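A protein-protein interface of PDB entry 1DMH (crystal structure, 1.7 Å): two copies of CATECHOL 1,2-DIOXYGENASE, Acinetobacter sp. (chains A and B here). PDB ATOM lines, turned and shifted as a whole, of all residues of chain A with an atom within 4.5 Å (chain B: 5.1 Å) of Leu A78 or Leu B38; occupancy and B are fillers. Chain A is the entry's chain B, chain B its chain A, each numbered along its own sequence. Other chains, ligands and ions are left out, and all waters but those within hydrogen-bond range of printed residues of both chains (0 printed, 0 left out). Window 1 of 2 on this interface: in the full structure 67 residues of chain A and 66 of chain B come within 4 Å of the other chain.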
ATOM      1  N   LEU A  74       4.939  24.313 -36.357  1.00  0.00           N
ATOM      2  CA  LEU A  74       4.720  24.628 -34.952  1.00  0.00           C
ATOM      3  C   LEU A  74       5.598  23.699 -34.100  1.00  0.00           C
ATOM      4  O   LEU A  74       6.147  24.105 -33.075  1.00  0.00           O
ATOM      5  CB  LEU A  74       3.244  24.384 -34.547  1.00  0.00           C
ATOM      6  CG  LEU A  74       2.550  25.164 -33.410  1.00  0.00           C
ATOM      7  CD1 LEU A  74       1.670  24.198 -32.670  1.00  0.00           C
ATOM      8  CD2 LEU A  74       3.517  25.894 -32.526  1.00  0.00           C
ATOM      9  N   SER A  75       5.720  22.444 -34.535  1.00  0.00           N
ATOM     10  CA  SER A  75       6.509  21.458 -33.821  1.00  0.00           C
ATOM     11  C   SER A  75       7.890  21.992 -33.423  1.00  0.00           C
ATOM     12  O   SER A  75       8.255  21.962 -32.248  1.00  0.00           O
ATOM     13  CB  SER A  75       6.647  20.188 -34.674  1.00  0.00           C
ATOM     14  OG  SER A  75       7.362  19.192 -33.978  1.00  0.00           O
ATOM     15  N   PRO A  76       8.704  22.442 -34.404  1.00  0.00           N
ATOM     16  CA  PRO A  76      10.013  22.960 -34.007  1.00  0.00           C
ATOM     17  C   PRO A  76       9.923  24.218 -33.163  1.00  0.00           C
ATOM     18  O   PRO A  76      10.748  24.430 -32.274  1.00  0.00           O
ATOM     19  CB  PRO A  76      10.724  23.176 -35.358  1.00  0.00           C
ATOM     20  CG  PRO A  76       9.566  23.412 -36.305  1.00  0.00           C
ATOM     21  CD  PRO A  76       8.610  22.353 -35.876  1.00  0.00           C
ATOM     22  N   GLY A  77       8.928  25.051 -33.444  1.00  0.00           N
ATOM     23  CA  GLY A  77       8.745  26.285 -32.684  1.00  0.00           C
ATOM     24  C   GLY A  77       8.449  25.996 -31.205  1.00  0.00           C
ATOM     25  O   GLY A  77       8.762  26.813 -30.342  1.00  0.00           O
ATOM     26  N   LEU A  78       7.857  24.834 -30.911  1.00  0.00           N
ATOM     27  CA  LEU A  78       7.560  24.467 -29.518  1.00  0.00           C
ATOM     28  C   LEU A  78       8.673  23.605 -28.923  1.00  0.00           C
ATOM     29  O   LEU A  78       8.508  23.018 -27.860  1.00  0.00           O
ATOM     30  CB  LEU A  78       6.187  23.769 -29.392  1.00  0.00           C
ATOM     31  CG  LEU A  78       4.975  24.667 -29.710  1.00  0.00           C
ATOM     32  CD1 LEU A  78       3.660  23.949 -29.431  1.00  0.00           C
ATOM     33  CD2 LEU A  78       5.060  25.925 -28.869  1.00  0.00           C
ATOM     34  N   GLY A  79       9.799  23.532 -29.630  1.00  0.00           N
ATOM     35  CA  GLY A  79      10.963  22.809 -29.141  1.00  0.00           C
ATOM     36  C   GLY A  79      11.055  21.295 -29.316  1.00  0.00           C
ATOM     37  O   GLY A  79      12.113  20.712 -29.038  1.00  0.00           O
ATOM     38  N   PHE A  80       9.984  20.652 -29.773  1.00  0.00           N
ATOM     39  CA  PHE A  80      10.045  19.207 -29.962  1.00  0.00           C
ATOM     40  C   PHE A  80      11.215  18.731 -30.827  1.00  0.00           C
ATOM     41  O   PHE A  80      11.930  17.788 -30.457  1.00  0.00           O
ATOM     42  CB  PHE A  80       8.734  18.650 -30.556  1.00  0.00           C
ATOM     43  CG  PHE A  80       7.547  18.745 -29.623  1.00  0.00           C
ATOM     44  CD1 PHE A  80       7.322  17.754 -28.664  1.00  0.00           C
ATOM     45  CD2 PHE A  80       6.681  19.840 -29.669  1.00  0.00           C
ATOM     46  CE1 PHE A  80       6.249  17.854 -27.762  1.00  0.00           C
ATOM     47  CE2 PHE A  80       5.603  19.944 -28.765  1.00  0.00           C
ATOM     48  CZ  PHE A  80       5.399  18.950 -27.823  1.00  0.00           C
ATOM     49  N   LEU A 211      -0.058  31.599 -32.567  1.00  0.00           N
ATOM     50  CA  LEU A 211       0.165  30.992 -31.262  1.00  0.00           C
ATOM     51  C   LEU A 211       1.458  31.600 -30.681  1.00  0.00           C
ATOM     52  O   LEU A 211       1.525  31.947 -29.504  1.00  0.00           O
ATOM     53  CB  LEU A 211       0.337  29.464 -31.382  1.00  0.00           C
ATOM     54  CG  LEU A 211       0.019  28.563 -30.171  1.00  0.00           C
ATOM     55  CD1 LEU A 211       0.813  27.266 -30.289  1.00  0.00           C
ATOM     56  CD2 LEU A 211       0.459  29.205 -28.934  1.00  0.00           C
ATOM     57  N   LEU A 215       2.550  33.806 -27.050  1.00  0.00           N
ATOM     58  CA  LEU A 215       3.611  33.445 -26.108  1.00  0.00           C
ATOM     59  C   LEU A 215       4.618  34.561 -26.009  1.00  0.00           C
ATOM     60  O   LEU A 215       5.649  34.438 -25.334  1.00  0.00           O
ATOM     61  CB  LEU A 215       4.321  32.168 -26.570  1.00  0.00           C
ATOM     62  CG  LEU A 215       3.422  30.933 -26.722  1.00  0.00           C
ATOM     63  CD1 LEU A 215       4.294  29.744 -27.145  1.00  0.00           C
ATOM     64  CD2 LEU A 215       2.694  30.641 -25.410  1.00  0.00           C
ATOM     65  N   LEU B  15      11.990  24.246 -21.521  1.00  0.00           N
ATOM     66  CA  LEU B  15      10.531  24.265 -21.503  1.00  0.00           C
ATOM     67  C   LEU B  15       9.994  25.651 -21.124  1.00  0.00           C
ATOM     68  O   LEU B  15       8.940  26.073 -21.607  1.00  0.00           O
ATOM     69  CB  LEU B  15      10.008  23.209 -20.516  1.00  0.00           C
ATOM     70  CG  LEU B  15      10.019  21.751 -20.999  1.00  0.00           C
ATOM     71  CD1 LEU B  15       9.830  20.780 -19.858  1.00  0.00           C
ATOM     72  CD2 LEU B  15       8.909  21.575 -22.037  1.00  0.00           C
ATOM     73  N   ALA B  18      10.609  27.960 -24.355  1.00  0.00           N
ATOM     74  CA  ALA B  18       9.668  27.624 -25.419  1.00  0.00           C
ATOM     75  C   ALA B  18       8.246  28.103 -25.115  1.00  0.00           C
ATOM     76  O   ALA B  18       7.498  28.467 -26.030  1.00  0.00           O
ATOM     77  CB  ALA B  18       9.676  26.125 -25.652  1.00  0.00           C
ATOM     78  N   SER B  19       7.867  28.101 -23.836  1.00  0.00           N
ATOM     79  CA  SER B  19       6.532  28.536 -23.436  1.00  0.00           C
ATOM     80  C   SER B  19       6.418  30.061 -23.292  1.00  0.00           C
ATOM     81  O   SER B  19       5.350  30.577 -22.948  1.00  0.00           O
ATOM     82  CB  SER B  19       6.150  27.869 -22.119  1.00  0.00           C
ATOM     83  OG  SER B  19       6.187  26.459 -22.271  1.00  0.00           O
ATOM     84  N   ILE B  33      -0.959  27.382 -19.874  1.00  0.00           N
ATOM     85  CA  ILE B  33      -1.466  26.130 -20.435  1.00  0.00           C
ATOM     86  C   ILE B  33      -0.396  25.455 -21.309  1.00  0.00           C
ATOM     87  O   ILE B  33      -0.126  24.258 -21.164  1.00  0.00           O
ATOM     88  CB  ILE B  33      -2.786  26.383 -21.231  1.00  0.00           C
ATOM     89  CG1 ILE B  33      -3.877  26.861 -20.248  1.00  0.00           C
ATOM     90  CG2 ILE B  33      -3.243  25.087 -22.000  1.00  0.00           C
ATOM     91  CD1 ILE B  33      -5.118  27.409 -20.941  1.00  0.00           C
ATOM     92  N   ILE B  34       0.232  26.227 -22.192  1.00  0.00           N
ATOM     93  CA  ILE B  34       1.273  25.691 -23.065  1.00  0.00           C
ATOM     94  C   ILE B  34       2.419  25.084 -22.262  1.00  0.00           C
ATOM     95  O   ILE B  34       2.875  23.976 -22.575  1.00  0.00           O
ATOM     96  CB  ILE B  34       1.837  26.776 -23.990  1.00  0.00           C
ATOM     97  CG1 ILE B  34       0.749  27.241 -24.958  1.00  0.00           C
ATOM     98  CG2 ILE B  34       3.028  26.226 -24.776  1.00  0.00           C
ATOM     99  CD1 ILE B  34       0.230  26.139 -25.847  1.00  0.00           C
ATOM    100  N   HIS B  35       2.888  25.781 -21.226  1.00  0.00           N
ATOM    101  CA  HIS B  35       3.970  25.228 -20.427  1.00  0.00           C
ATOM    102  C   HIS B  35       3.592  23.860 -19.849  1.00  0.00           C
ATOM    103  O   HIS B  35       4.376  22.923 -19.902  1.00  0.00           O
ATOM    104  CB  HIS B  35       4.364  26.181 -19.303  1.00  0.00           C
ATOM    105  CG  HIS B  35       5.535  25.701 -18.506  1.00  0.00           C
ATOM    106  ND1 HIS B  35       5.409  25.187 -17.233  1.00  0.00           N
ATOM    107  CD2 HIS B  35       6.837  25.551 -18.846  1.00  0.00           C
ATOM    108  CE1 HIS B  35       6.581  24.736 -16.824  1.00  0.00           C
ATOM    109  NE2 HIS B  35       7.464  24.945 -17.784  1.00  0.00           N
ATOM    110  N   ARG B  36       2.384  23.728 -19.325  1.00  0.00           N
ATOM    111  CA  ARG B  36       1.961  22.449 -18.762  1.00  0.00           C
ATOM    112  C   ARG B  36       1.825  21.356 -19.816  1.00  0.00           C
ATOM    113  O   ARG B  36       2.304  20.242 -19.628  1.00  0.00           O
ATOM    114  CB  ARG B  36       0.629  22.621 -18.022  1.00  0.00           C
ATOM    115  CG  ARG B  36      -0.043  21.330 -17.576  1.00  0.00           C
ATOM    116  CD  ARG B  36       0.818  20.506 -16.657  1.00  0.00           C
ATOM    117  NE  ARG B  36       0.044  19.389 -16.126  1.00  0.00           N
ATOM    118  CZ  ARG B  36      -0.757  19.479 -15.065  1.00  0.00           C
ATOM    119  NH1 ARG B  36      -0.874  20.634 -14.404  1.00  0.00           N
ATOM    120  NH2 ARG B  36      -1.496  18.443 -14.707  1.00  0.00           N
ATOM    121  N   VAL B  37       1.165  21.663 -20.928  1.00  0.00           N
ATOM    122  CA  VAL B  37       1.001  20.667 -21.973  1.00  0.00           C
ATOM    123  C   VAL B  37       2.357  20.219 -22.543  1.00  0.00           C
ATOM    124  O   VAL B  37       2.568  19.027 -22.748  1.00  0.00           O
ATOM    125  CB  VAL B  37       0.076  21.190 -23.107  1.00  0.00           C
ATOM    126  CG1 VAL B  37      -0.021  20.146 -24.220  1.00  0.00           C
ATOM    127  CG2 VAL B  37      -1.311  21.459 -22.556  1.00  0.00           C
ATOM    128  N   LEU B  38       3.280  21.150 -22.789  1.00  0.00           N
ATOM    129  CA  LEU B  38       4.604  20.763 -23.314  1.00  0.00           C
ATOM    130  C   LEU B  38       5.378  19.911 -22.320  1.00  0.00           C
ATOM    131  O   LEU B  38       6.031  18.943 -22.686  1.00  0.00           O
ATOM    132  CB  LEU B  38       5.476  21.974 -23.636  1.00  0.00           C
ATOM    133  CG  LEU B  38       5.054  22.855 -24.799  1.00  0.00           C
ATOM    134  CD1 LEU B  38       6.094  23.940 -24.996  1.00  0.00           C
ATOM    135  CD2 LEU B  38       4.940  22.005 -26.038  1.00  0.00           C
ATOM    136  N   SER B  39       5.325  20.297 -21.056  1.00  0.00           N
ATOM    137  CA  SER B  39       6.022  19.553 -20.028  1.00  0.00           C
ATOM    138  C   SER B  39       5.511  18.134 -19.999  1.00  0.00           C
ATOM    139  O   SER B  39       6.291  17.197 -20.013  1.00  0.00           O
ATOM    140  CB  SER B  39       5.816  20.209 -18.662  1.00  0.00           C
ATOM    141  OG  SER B  39       6.426  21.486 -18.666  1.00  0.00           O
ATOM    142  N   ASP B  40       4.200  17.974 -19.951  1.00  0.00           N
ATOM    143  CA  ASP B  40       3.633  16.631 -19.925  1.00  0.00           C
ATOM    144  C   ASP B  40       4.018  15.812 -21.164  1.00  0.00           C
ATOM    145  O   ASP B  40       4.340  14.641 -21.050  1.00  0.00           O
ATOM    146  CB  ASP B  40       2.096  16.676 -19.788  1.00  0.00           C
ATOM    147  CG  ASP B  40       1.633  17.132 -18.397  1.00  0.00           C
ATOM    148  OD1 ASP B  40       2.438  17.148 -17.434  1.00  0.00           O
ATOM    149  OD2 ASP B  40       0.443  17.460 -18.280  1.00  0.00           O
ATOM    150  N   LEU B  41       3.990  16.423 -22.346  1.00  0.00           N
ATOM    151  CA  LEU B  41       4.338  15.691 -23.557  1.00  0.00           C
ATOM    152  C   LEU B  41       5.815  15.332 -23.625  1.00  0.00           C
ATOM    153  O   LEU B  41       6.156  14.240 -24.073  1.00  0.00           O
ATOM    154  CB  LEU B  41       3.931  16.487 -24.803  1.00  0.00           C
ATOM    155  CG  LEU B  41       2.433  16.529 -25.090  1.00  0.00           C
ATOM    156  CD1 LEU B  41       2.188  17.460 -26.277  1.00  0.00           C
ATOM    157  CD2 LEU B  41       1.927  15.132 -25.402  1.00  0.00           C
ATOM    158  N   TYR B  42       6.687  16.250 -23.215  1.00  0.00           N
ATOM    159  CA  TYR B  42       8.127  15.968 -23.213  1.00  0.00           C
ATOM    160  C   TYR B  42       8.368  14.810 -22.251  1.00  0.00           C
ATOM    161  O   TYR B  42       9.166  13.921 -22.528  1.00  0.00           O
ATOM    162  CB  TYR B  42       8.934  17.177 -22.738  1.00  0.00           C
ATOM    163  CG  TYR B  42       9.301  18.192 -23.803  1.00  0.00           C
ATOM    164  CD1 TYR B  42       8.379  18.590 -24.778  1.00  0.00           C
ATOM    165  CD2 TYR B  42      10.522  18.855 -23.746  1.00  0.00           C
ATOM    166  CE1 TYR B  42       8.663  19.635 -25.641  1.00  0.00           C
ATOM    167  CE2 TYR B  42      10.816  19.904 -24.609  1.00  0.00           C
ATOM    168  CZ  TYR B  42       9.882  20.293 -25.541  1.00  0.00           C
ATOM    169  OH  TYR B  42      10.124  21.395 -26.311  1.00  0.00           O
ATOM    170  N   LYS B  43       7.682  14.821 -21.113  1.00  0.00           N
ATOM    171  CA  LYS B  43       7.854  13.734 -20.166  1.00  0.00           C
ATOM    172  C   LYS B  43       7.271  12.436 -20.732  1.00  0.00           C
ATOM    173  O   LYS B  43       7.874  11.382 -20.560  1.00  0.00           O
ATOM    174  CB  LYS B  43       7.195  14.080 -18.829  1.00  0.00           C
ATOM    175  CG  LYS B  43       7.469  13.074 -17.742  1.00  0.00           C
ATOM    176  CD  LYS B  43       6.883  13.556 -16.442  1.00  0.00           C
ATOM    177  CE  LYS B  43       7.292  12.670 -15.256  1.00  0.00           C
ATOM    178  NZ  LYS B  43       6.770  11.269 -15.389  1.00  0.00           N
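Leu A78 touches Ala B18 (O to CB, 3.99 Å).
Leu B38 touches Leu A78.
Leu B38 touches Phe A80 (CD2 to CE2, 3.5 Å).
CD1 of Leu B41 touches CZ of Phe A80, 3.9 Å away.
Phe A80 touches Tyr B42 (N to OH, 3.5 Å).
Ala B18 touches Leu A215.
O of Ser B19 touches CD2 of Leu A215 (3.6 Å).
CG1 of Ile B34 touches CD2 of Leu A215, at 3.9 Å.
No position is printed for both chains.
The backbone carbonyl oxygen of Leu B15 sits at hydrogen-bond distance from the side-chain hydroxyl of Ser B19 (2.9 Å).
The backbone NH of Phe A80 is in hydrogen-bond range of the backbone carbonyl oxygen of Ser A75 (3.3 Å).
The side-chain hydroxyl (OH) of Tyr B42 lies close to the backbone carbonyl oxygen (O) of Gly A79 (3.4 Å).
The side-chain hydroxyl (OH) of Tyr B42 is in hydrogen-bond range of the backbone carbonyl oxygen (O) of Leu A78 (2.8 Å).
Of the 9 printed residues of chain A, 4 touch a printed residue of chain B.
Hydrophobic or aromatic side chains of chain B within 4 Å of the printed part of chain A: Ala B18, Ile B34, Leu B38, Leu B41 and Tyr B42.
Among the printed residues, no Asp or Glu carboxylate lies within 4 Å of a Lys or Arg side-chain nitrogen of the other chain.
Printed residues of chain B within 4 Å of Leu A78: Ala B18, Leu B38 and Tyr B42.
Of the printed residues of chain B, Leu A215 touches Ala B18 (3.6 Å), Ser B19 (3.6 Å) and Ile B34 (3.9 Å).
Printed residues of chain A within 4 Å of Ile B34: Leu A215.
Leu B38 touches just these residues of chain A: Leu A78 and Phe A80.
Of the printed residues of chain A, Leu B41 touches Phe A80 (3.9 Å).
The nearest printed residue of chain A that does not touch Leu B38 is Gly A79 (5.9 Å).
The nearest printed residue of chain A that does not touch Tyr B42 is Ser A75 (6.3 Å).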
